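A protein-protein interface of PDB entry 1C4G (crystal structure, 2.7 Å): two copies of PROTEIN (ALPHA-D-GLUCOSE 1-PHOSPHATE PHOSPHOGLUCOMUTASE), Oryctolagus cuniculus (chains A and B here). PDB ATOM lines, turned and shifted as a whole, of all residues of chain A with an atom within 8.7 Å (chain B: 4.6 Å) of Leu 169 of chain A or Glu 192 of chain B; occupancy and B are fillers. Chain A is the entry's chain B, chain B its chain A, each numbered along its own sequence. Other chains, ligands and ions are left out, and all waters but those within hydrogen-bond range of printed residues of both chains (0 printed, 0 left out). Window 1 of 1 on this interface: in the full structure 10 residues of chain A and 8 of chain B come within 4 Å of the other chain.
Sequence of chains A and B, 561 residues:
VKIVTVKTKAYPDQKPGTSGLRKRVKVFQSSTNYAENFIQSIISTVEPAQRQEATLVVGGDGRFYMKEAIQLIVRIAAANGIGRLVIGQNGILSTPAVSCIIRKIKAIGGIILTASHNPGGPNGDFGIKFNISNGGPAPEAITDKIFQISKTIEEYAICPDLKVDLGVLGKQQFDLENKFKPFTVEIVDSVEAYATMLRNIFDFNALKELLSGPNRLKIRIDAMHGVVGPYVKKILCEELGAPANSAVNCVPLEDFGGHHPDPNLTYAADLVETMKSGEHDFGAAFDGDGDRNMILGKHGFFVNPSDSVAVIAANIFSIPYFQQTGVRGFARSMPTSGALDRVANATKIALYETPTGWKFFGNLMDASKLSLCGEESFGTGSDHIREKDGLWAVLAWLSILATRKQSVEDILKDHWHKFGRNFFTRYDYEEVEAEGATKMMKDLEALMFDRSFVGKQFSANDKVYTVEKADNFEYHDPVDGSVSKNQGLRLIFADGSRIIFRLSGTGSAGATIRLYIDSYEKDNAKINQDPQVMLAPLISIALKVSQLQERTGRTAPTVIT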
ATOM      1  N   ILE A  87     -12.720 -21.413 -29.659  1.00  0.00           N
ATOM      2  CA  ILE A  87     -12.751 -20.427 -28.586  1.00  0.00           C
ATOM      3  C   ILE A  87     -12.616 -21.079 -27.187  1.00  0.00           C
ATOM      4  O   ILE A  87     -13.178 -22.109 -26.912  1.00  0.00           O
ATOM      5  CB  ILE A  87     -14.090 -19.607 -28.677  1.00  0.00           C
ATOM      6  CG1 ILE A  87     -14.315 -19.150 -30.099  1.00  0.00           C
ATOM      7  CG2 ILE A  87     -14.113 -18.405 -27.721  1.00  0.00           C
ATOM      8  CD1 ILE A  87     -15.605 -18.349 -30.235  1.00  0.00           C
ATOM      9  N   GLY A  88     -11.850 -20.508 -26.304  1.00  0.00           N
ATOM     10  CA  GLY A  88     -11.755 -21.056 -25.003  1.00  0.00           C
ATOM     11  C   GLY A  88     -13.075 -20.891 -24.223  1.00  0.00           C
ATOM     12  O   GLY A  88     -13.973 -20.131 -24.630  1.00  0.00           O
ATOM     13  N   GLN A  89     -13.185 -21.533 -23.023  1.00  0.00           N
ATOM     14  CA  GLN A  89     -14.413 -21.458 -22.239  1.00  0.00           C
ATOM     15  C   GLN A  89     -14.647 -20.089 -21.638  1.00  0.00           C
ATOM     16  O   GLN A  89     -13.857 -19.594 -20.837  1.00  0.00           O
ATOM     17  CB  GLN A  89     -14.426 -22.500 -21.140  1.00  0.00           C
ATOM     18  CG  GLN A  89     -15.849 -22.758 -20.621  1.00  0.00           C
ATOM     19  CD  GLN A  89     -15.885 -23.639 -19.377  1.00  0.00           C
ATOM     20  OE1 GLN A  89     -14.880 -24.058 -18.884  1.00  0.00           O
ATOM     21  NE2 GLN A  89     -17.041 -23.953 -18.848  1.00  0.00           N
ATOM     22  N   ASN A  90     -15.798 -19.477 -22.030  1.00  0.00           N
ATOM     23  CA  ASN A  90     -16.210 -18.099 -21.600  1.00  0.00           C
ATOM     24  C   ASN A  90     -15.422 -17.024 -22.316  1.00  0.00           C
ATOM     25  O   ASN A  90     -15.623 -15.832 -22.134  1.00  0.00           O
ATOM     26  CB  ASN A  90     -16.118 -17.904 -20.076  1.00  0.00           C
ATOM     27  CG  ASN A  90     -17.204 -18.655 -19.330  1.00  0.00           C
ATOM     28  OD1 ASN A  90     -16.947 -19.618 -18.661  1.00  0.00           O
ATOM     29  ND2 ASN A  90     -18.452 -18.252 -19.436  1.00  0.00           N
ATOM     30  N   ASP A 165     -23.289 -19.482 -27.769  1.00  0.00           N
ATOM     31  CA  ASP A 165     -23.214 -19.654 -26.323  1.00  0.00           C
ATOM     32  C   ASP A 165     -21.778 -20.054 -25.951  1.00  0.00           C
ATOM     33  O   ASP A 165     -21.372 -21.194 -26.037  1.00  0.00           O
ATOM     34  CB  ASP A 165     -24.197 -20.716 -25.849  1.00  0.00           C
ATOM     35  CG  ASP A 165     -24.772 -20.473 -24.398  1.00  0.00           C
ATOM     36  OD1 ASP A 165     -24.188 -19.694 -23.596  1.00  0.00           O
ATOM     37  OD2 ASP A 165     -25.806 -21.073 -24.082  1.00  0.00           O
ATOM     38  N   LEU A 166     -21.007 -19.083 -25.518  1.00  0.00           N
ATOM     39  CA  LEU A 166     -19.573 -19.259 -25.206  1.00  0.00           C
ATOM     40  C   LEU A 166     -19.252 -20.027 -23.929  1.00  0.00           C
ATOM     41  O   LEU A 166     -18.132 -20.452 -23.723  1.00  0.00           O
ATOM     42  CB  LEU A 166     -18.984 -17.871 -25.041  1.00  0.00           C
ATOM     43  CG  LEU A 166     -18.269 -17.215 -26.196  1.00  0.00           C
ATOM     44  CD1 LEU A 166     -19.123 -17.162 -27.445  1.00  0.00           C
ATOM     45  CD2 LEU A 166     -17.865 -15.836 -25.773  1.00  0.00           C
ATOM     46  N   GLY A 167     -20.185 -20.165 -23.026  1.00  0.00           N
ATOM     47  CA  GLY A 167     -19.864 -20.811 -21.752  1.00  0.00           C
ATOM     48  C   GLY A 167     -20.017 -22.318 -21.746  1.00  0.00           C
ATOM     49  O   GLY A 167     -19.525 -23.007 -20.831  1.00  0.00           O
ATOM     50  N   VAL A 168     -20.680 -22.888 -22.754  1.00  0.00           N
ATOM     51  CA  VAL A 168     -20.889 -24.327 -22.760  1.00  0.00           C
ATOM     52  C   VAL A 168     -19.897 -25.124 -23.674  1.00  0.00           C
ATOM     53  O   VAL A 168     -19.842 -24.947 -24.879  1.00  0.00           O
ATOM     54  CB  VAL A 168     -22.391 -24.629 -23.056  1.00  0.00           C
ATOM     55  CG1 VAL A 168     -22.891 -23.956 -24.310  1.00  0.00           C
ATOM     56  CG2 VAL A 168     -22.593 -26.105 -23.157  1.00  0.00           C
ATOM     57  N   LEU A 169     -19.093 -26.034 -23.070  1.00  0.00           N
ATOM     58  CA  LEU A 169     -18.083 -26.813 -23.843  1.00  0.00           C
ATOM     59  C   LEU A 169     -18.647 -27.616 -25.032  1.00  0.00           C
ATOM     60  O   LEU A 169     -19.778 -28.127 -24.994  1.00  0.00           O
ATOM     61  CB  LEU A 169     -17.336 -27.765 -22.911  1.00  0.00           C
ATOM     62  CG  LEU A 169     -16.000 -27.283 -22.366  1.00  0.00           C
ATOM     63  CD1 LEU A 169     -15.927 -27.403 -20.852  1.00  0.00           C
ATOM     64  CD2 LEU A 169     -14.888 -28.062 -22.989  1.00  0.00           C
ATOM     65  N   GLY A 170     -17.870 -27.783 -26.105  1.00  0.00           N
ATOM     66  CA  GLY A 170     -18.378 -28.544 -27.203  1.00  0.00           C
ATOM     67  C   GLY A 170     -18.531 -27.775 -28.481  1.00  0.00           C
ATOM     68  O   GLY A 170     -18.512 -26.533 -28.543  1.00  0.00           O
ATOM     69  N   LYS A 171     -18.732 -28.565 -29.523  1.00  0.00           N
ATOM     70  CA  LYS A 171     -18.876 -28.113 -30.920  1.00  0.00           C
ATOM     71  C   LYS A 171     -20.289 -27.591 -31.284  1.00  0.00           C
ATOM     72  O   LYS A 171     -21.247 -28.329 -31.349  1.00  0.00           O
ATOM     73  CB  LYS A 171     -18.540 -29.339 -31.802  1.00  0.00           C
ATOM     74  CG  LYS A 171     -17.704 -29.047 -33.004  1.00  0.00           C
ATOM     75  CD  LYS A 171     -16.661 -30.131 -33.169  1.00  0.00           C
ATOM     76  CE  LYS A 171     -16.426 -30.388 -34.671  1.00  0.00           C
ATOM     77  NZ  LYS A 171     -15.294 -31.305 -34.896  1.00  0.00           N
ATOM     78  N   GLN A 172     -20.436 -26.322 -31.471  1.00  0.00           N
ATOM     79  CA  GLN A 172     -21.715 -25.773 -31.906  1.00  0.00           C
ATOM     80  C   GLN A 172     -21.702 -25.569 -33.426  1.00  0.00           C
ATOM     81  O   GLN A 172     -20.727 -25.065 -34.001  1.00  0.00           O
ATOM     82  CB  GLN A 172     -21.986 -24.442 -31.217  1.00  0.00           C
ATOM     83  CG  GLN A 172     -22.321 -24.626 -29.734  1.00  0.00           C
ATOM     84  CD  GLN A 172     -22.387 -23.327 -28.920  1.00  0.00           C
ATOM     85  OE1 GLN A 172     -22.972 -22.336 -29.315  1.00  0.00           O
ATOM     86  NE2 GLN A 172     -21.808 -23.323 -27.762  1.00  0.00           N
ATOM     87  N   VAL A 185     -18.195 -23.730 -34.499  1.00  0.00           N
ATOM     88  CA  VAL A 185     -17.627 -23.000 -33.337  1.00  0.00           C
ATOM     89  C   VAL A 185     -17.308 -24.033 -32.278  1.00  0.00           C
ATOM     90  O   VAL A 185     -18.199 -24.674 -31.718  1.00  0.00           O
ATOM     91  CB  VAL A 185     -18.601 -22.016 -32.705  1.00  0.00           C
ATOM     92  CG1 VAL A 185     -17.845 -21.061 -31.818  1.00  0.00           C
ATOM     93  CG2 VAL A 185     -19.373 -21.242 -33.744  1.00  0.00           C
ATOM     94  N   GLU A 186     -16.065 -24.223 -31.955  1.00  0.00           N
ATOM     95  CA  GLU A 186     -15.724 -25.247 -31.004  1.00  0.00           C
ATOM     96  C   GLU A 186     -15.270 -24.719 -29.630  1.00  0.00           C
ATOM     97  O   GLU A 186     -14.168 -24.251 -29.495  1.00  0.00           O
ATOM     98  CB  GLU A 186     -14.648 -26.032 -31.638  1.00  0.00           C
ATOM     99  CG  GLU A 186     -14.300 -27.305 -30.926  1.00  0.00           C
ATOM    100  CD  GLU A 186     -13.324 -28.060 -31.733  1.00  0.00           C
ATOM    101  OE1 GLU A 186     -12.278 -28.390 -31.196  1.00  0.00           O
ATOM    102  OE2 GLU A 186     -13.597 -28.289 -32.935  1.00  0.00           O
ATOM    103  N   ILE A 187     -16.099 -24.794 -28.570  1.00  0.00           N
ATOM    104  CA  ILE A 187     -15.622 -24.284 -27.276  1.00  0.00           C
ATOM    105  C   ILE A 187     -14.740 -25.292 -26.496  1.00  0.00           C
ATOM    106  O   ILE A 187     -15.127 -26.452 -26.176  1.00  0.00           O
ATOM    107  CB  ILE A 187     -16.752 -23.648 -26.421  1.00  0.00           C
ATOM    108  CG1 ILE A 187     -17.071 -22.232 -26.993  1.00  0.00           C
ATOM    109  CG2 ILE A 187     -16.321 -23.499 -24.950  1.00  0.00           C
ATOM    110  CD1 ILE A 187     -17.550 -22.180 -28.463  1.00  0.00           C
ATOM    111  N   VAL A 188     -13.507 -24.823 -26.222  1.00  0.00           N
ATOM    112  CA  VAL A 188     -12.467 -25.612 -25.598  1.00  0.00           C
ATOM    113  C   VAL A 188     -12.243 -25.232 -24.118  1.00  0.00           C
ATOM    114  O   VAL A 188     -12.604 -24.136 -23.668  1.00  0.00           O
ATOM    115  CB  VAL A 188     -11.159 -25.369 -26.436  1.00  0.00           C
ATOM    116  CG1 VAL A 188      -9.899 -25.678 -25.662  1.00  0.00           C
ATOM    117  CG2 VAL A 188     -11.190 -26.160 -27.730  1.00  0.00           C
ATOM    118  N   ASP A 189     -11.710 -26.172 -23.310  1.00  0.00           N
ATOM    119  CA  ASP A 189     -11.391 -25.871 -21.933  1.00  0.00           C
ATOM    120  C   ASP A 189     -10.244 -24.876 -21.866  1.00  0.00           C
ATOM    121  O   ASP A 189      -9.230 -25.069 -22.517  1.00  0.00           O
ATOM    122  CB  ASP A 189     -10.939 -27.101 -21.265  1.00  0.00           C
ATOM    123  CG  ASP A 189     -10.898 -26.929 -19.794  1.00  0.00           C
ATOM    124  OD1 ASP A 189      -9.803 -27.042 -19.203  1.00  0.00           O
ATOM    125  OD2 ASP A 189     -11.976 -26.675 -19.213  1.00  0.00           O
ATOM    126  N   SER A 190     -10.337 -23.836 -21.048  1.00  0.00           N
ATOM    127  CA  SER A 190      -9.249 -22.850 -20.976  1.00  0.00           C
ATOM    128  C   SER A 190      -7.895 -23.447 -20.637  1.00  0.00           C
ATOM    129  O   SER A 190      -6.929 -23.247 -21.353  1.00  0.00           O
ATOM    130  CB  SER A 190      -9.555 -21.765 -19.969  1.00  0.00           C
ATOM    131  OG  SER A 190     -10.818 -21.163 -20.213  1.00  0.00           O
ATOM    132  N   GLU A 192      -6.768 -26.997 -20.110  1.00  0.00           N
ATOM    133  CA  GLU A 192      -6.419 -28.289 -20.783  1.00  0.00           C
ATOM    134  C   GLU A 192      -5.192 -28.363 -21.754  1.00  0.00           C
ATOM    135  O   GLU A 192      -4.133 -28.840 -21.356  1.00  0.00           O
ATOM    136  CB  GLU A 192      -7.679 -28.864 -21.454  1.00  0.00           C
ATOM    137  CG  GLU A 192      -7.714 -30.392 -21.427  1.00  0.00           C
ATOM    138  CD  GLU A 192      -6.998 -30.963 -22.598  1.00  0.00           C
ATOM    139  OE1 GLU A 192      -7.558 -30.930 -23.686  1.00  0.00           O
ATOM    140  OE2 GLU A 192      -5.862 -31.403 -22.443  1.00  0.00           O
ATOM    141  N   ASP B 189     -14.000 -34.502 -20.694  1.00  0.00           N
ATOM    142  CA  ASP B 189     -15.118 -33.957 -19.846  1.00  0.00           C
ATOM    143  C   ASP B 189     -16.313 -34.977 -19.934  1.00  0.00           C
ATOM    144  O   ASP B 189     -16.547 -35.611 -20.991  1.00  0.00           O
ATOM    145  CB  ASP B 189     -15.582 -32.547 -20.358  1.00  0.00           C
ATOM    146  CG  ASP B 189     -16.523 -31.721 -19.382  1.00  0.00           C
ATOM    147  OD1 ASP B 189     -16.033 -30.866 -18.621  1.00  0.00           O
ATOM    148  OD2 ASP B 189     -17.729 -31.895 -19.431  1.00  0.00           O
ATOM    149  N   SER B 190     -17.080 -35.148 -18.838  1.00  0.00           N
ATOM    150  CA  SER B 190     -18.206 -36.103 -18.832  1.00  0.00           C
ATOM    151  C   SER B 190     -19.361 -35.742 -19.793  1.00  0.00           C
ATOM    152  O   SER B 190     -19.831 -36.545 -20.586  1.00  0.00           O
ATOM    153  CB  SER B 190     -18.786 -36.189 -17.440  1.00  0.00           C
ATOM    154  OG  SER B 190     -17.781 -36.385 -16.457  1.00  0.00           O
ATOM    155  N   VAL B 191     -19.815 -34.514 -19.740  1.00  0.00           N
ATOM    156  CA  VAL B 191     -20.969 -34.060 -20.528  1.00  0.00           C
ATOM    157  C   VAL B 191     -20.682 -33.676 -21.982  1.00  0.00           C
ATOM    158  O   VAL B 191     -21.461 -33.991 -22.869  1.00  0.00           O
ATOM    159  CB  VAL B 191     -21.504 -32.853 -19.803  1.00  0.00           C
ATOM    160  CG1 VAL B 191     -22.690 -32.256 -20.521  1.00  0.00           C
ATOM    161  CG2 VAL B 191     -21.820 -33.212 -18.339  1.00  0.00           C
ATOM    162  N   GLU B 192     -19.511 -33.014 -22.242  1.00  0.00           N
ATOM    163  CA  GLU B 192     -19.163 -32.435 -23.592  1.00  0.00           C
ATOM    164  C   GLU B 192     -19.637 -33.157 -24.882  1.00  0.00           C
ATOM    165  O   GLU B 192     -20.518 -32.661 -25.602  1.00  0.00           O
ATOM    166  CB  GLU B 192     -17.684 -32.207 -23.676  1.00  0.00           C
ATOM    167  CG  GLU B 192     -17.323 -31.186 -24.745  1.00  0.00           C
ATOM    168  CD  GLU B 192     -16.883 -31.832 -26.037  1.00  0.00           C
ATOM    169  OE1 GLU B 192     -15.738 -32.262 -26.104  1.00  0.00           O
ATOM    170  OE2 GLU B 192     -17.696 -31.925 -26.980  1.00  0.00           O
ATOM    171  N   ALA B 193     -18.971 -34.274 -25.279  1.00  0.00           N
ATOM    172  CA  ALA B 193     -19.373 -34.998 -26.509  1.00  0.00           C
ATOM    173  C   ALA B 193     -20.858 -35.364 -26.507  1.00  0.00           C
ATOM    174  O   ALA B 193     -21.570 -35.180 -27.507  1.00  0.00           O
ATOM    175  CB  ALA B 193     -18.597 -36.292 -26.617  1.00  0.00           C
ATOM    176  N   TYR B 194     -21.376 -35.824 -25.365  1.00  0.00           N
ATOM    177  CA  TYR B 194     -22.770 -36.170 -25.282  1.00  0.00           C
ATOM    178  C   TYR B 194     -23.663 -34.929 -25.598  1.00  0.00           C
ATOM    179  O   TYR B 194     -24.575 -35.013 -26.392  1.00  0.00           O
ATOM    180  CB  TYR B 194     -23.052 -36.746 -23.885  1.00  0.00           C
ATOM    181  CG  TYR B 194     -24.490 -37.005 -23.644  1.00  0.00           C
ATOM    182  CD1 TYR B 194     -25.184 -36.227 -22.735  1.00  0.00           C
ATOM    183  CD2 TYR B 194     -25.143 -38.000 -24.364  1.00  0.00           C
ATOM    184  CE1 TYR B 194     -26.552 -36.432 -22.537  1.00  0.00           C
ATOM    185  CE2 TYR B 194     -26.503 -38.211 -24.181  1.00  0.00           C
ATOM    186  CZ  TYR B 194     -27.204 -37.417 -23.265  1.00  0.00           C
ATOM    187  OH  TYR B 194     -28.587 -37.573 -23.136  1.00  0.00           O
ATOM    188  N   ALA B 195     -23.356 -33.744 -25.043  1.00  0.00           N
ATOM    189  CA  ALA B 195     -24.168 -32.532 -25.351  1.00  0.00           C
ATOM    190  C   ALA B 195     -23.997 -32.119 -26.785  1.00  0.00           C
ATOM    191  O   ALA B 195     -24.946 -31.776 -27.450  1.00  0.00           O
ATOM    192  CB  ALA B 195     -23.730 -31.362 -24.510  1.00  0.00           C
ATOM    193  N   THR B 196     -22.788 -32.180 -27.317  1.00  0.00           N
ATOM    194  CA  THR B 196     -22.579 -31.857 -28.737  1.00  0.00           C
ATOM    195  C   THR B 196     -23.418 -32.807 -29.603  1.00  0.00           C
ATOM    196  O   THR B 196     -23.885 -32.450 -30.646  1.00  0.00           O
ATOM    197  CB  THR B 196     -21.090 -32.014 -29.103  1.00  0.00           C
ATOM    198  OG1 THR B 196     -20.378 -31.160 -28.240  1.00  0.00           O
ATOM    199  CG2 THR B 196     -20.802 -31.643 -30.525  1.00  0.00           C
ATOM    200  N   ARG B 199     -27.106 -31.744 -29.354  1.00  0.00           N
ATOM    201  CA  ARG B 199     -27.167 -30.432 -30.064  1.00  0.00           C
ATOM    202  C   ARG B 199     -27.631 -30.554 -31.516  1.00  0.00           C
ATOM    203  O   ARG B 199     -28.452 -29.788 -31.974  1.00  0.00           O
ATOM    204  CB  ARG B 199     -25.807 -29.857 -30.067  1.00  0.00           C
ATOM    205  CG  ARG B 199     -25.802 -28.374 -29.893  1.00  0.00           C
ATOM    206  CD  ARG B 199     -25.282 -28.010 -28.521  1.00  0.00           C
ATOM    207  NE  ARG B 199     -23.983 -28.572 -28.308  1.00  0.00           N
ATOM    208  CZ  ARG B 199     -23.244 -28.168 -27.296  1.00  0.00           C
ATOM    209  NH1 ARG B 199     -23.707 -27.226 -26.455  1.00  0.00           N
ATOM    210  NH2 ARG B 199     -21.999 -28.699 -27.118  1.00  0.00           N
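The backbone NH of Lys 171 of chain A sits at hydrogen-bond distance from the side-chain hydroxyl of Thr 196 of chain B, at 3.3 Å. NH2 of Arg 199 of chain B is in hydrogen-bond range of O of Leu 169 of chain A (3.1 Å).
Of the 19 printed residues of chain A, 4 touch a printed residue of chain B. Printed residues of chain A that touch a printed residue of chain B: Val 168, Leu 169, Gly 170 and Lys 171. Along chain B the printed residues that touch a printed residue of chain A span positions 192 to 199.
3 positions are printed for both chains. Of the 7 pairs that touch across the chains among the printed residues, none has its exchanged pair printed and touching as well.
The backbone carbonyl oxygen (O) of Glu 192 of chain B is in hydrogen-bond range of the side-chain hydroxyl (OG1) of Thr 196 of chain B (3.0 Å). O of Ala 195 of chain B lies close to NE of Arg 199 of chain B (3.5 Å). The side-chain hydroxyl (OG1) of Thr 196 of chain B sits at hydrogen-bond distance from the guanidinium group (NH2) of Arg 199 of chain B, 3.2 Å away. The backbone carbonyl oxygen (O) of Gly 170 of chain A lies within hydrogen-bond range of the backbone NH (N) of Ile 187 of chain A, at 3.0 Å. NZ of Lys 171 of chain A is in salt-bridge range of OE2 of Glu 186 of chain A.
Among the printed residues, pairs that only touch across the chains: Val 168 of chain A with Arg 199 of chain B (3.7 Å), Leu 169 of chain A with Glu 192 of chain B (3.8 Å), Gly 170 of chain A with Glu 192 of chain B (3.5 Å), Gly 170 of chain A with Thr 196 of chain B (3.5 Å) and Gly 170 of chain A with Arg 199 of chain B (3.6 Å).
Printed residues of chain B within 4 Å of Gly 170 of chain A: Glu 192 (3.5 Å), Thr 196 (3.5 Å) and Arg 199 (3.6 Å). Ser 190 of chain A touches none of the printed residues of chain B. Asp 189 of chain B touches none of the printed residues of chain A. No residue of chain A comes within 4 Å of Val 191 of chain B. Glu 192 of chain B touches just these residues of chain A: Leu 169 and Gly 170. Of the printed residues of chain A, Thr 196 of chain B touches Gly 170 (3.5 Å) and Lys 171 (3.3 Å). Printed residues of chain A within 4 Å of Arg 199 of chain B: Val 168, Leu 169 and Gly 170. The nearest residue of chain B that does not touch Leu 169 of chain A is Asp 189 of chain B (4.1 Å). The nearest printed residue of chain B that does not touch Val 168 of chain A is Ala 195 of chain B (5.5 Å).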
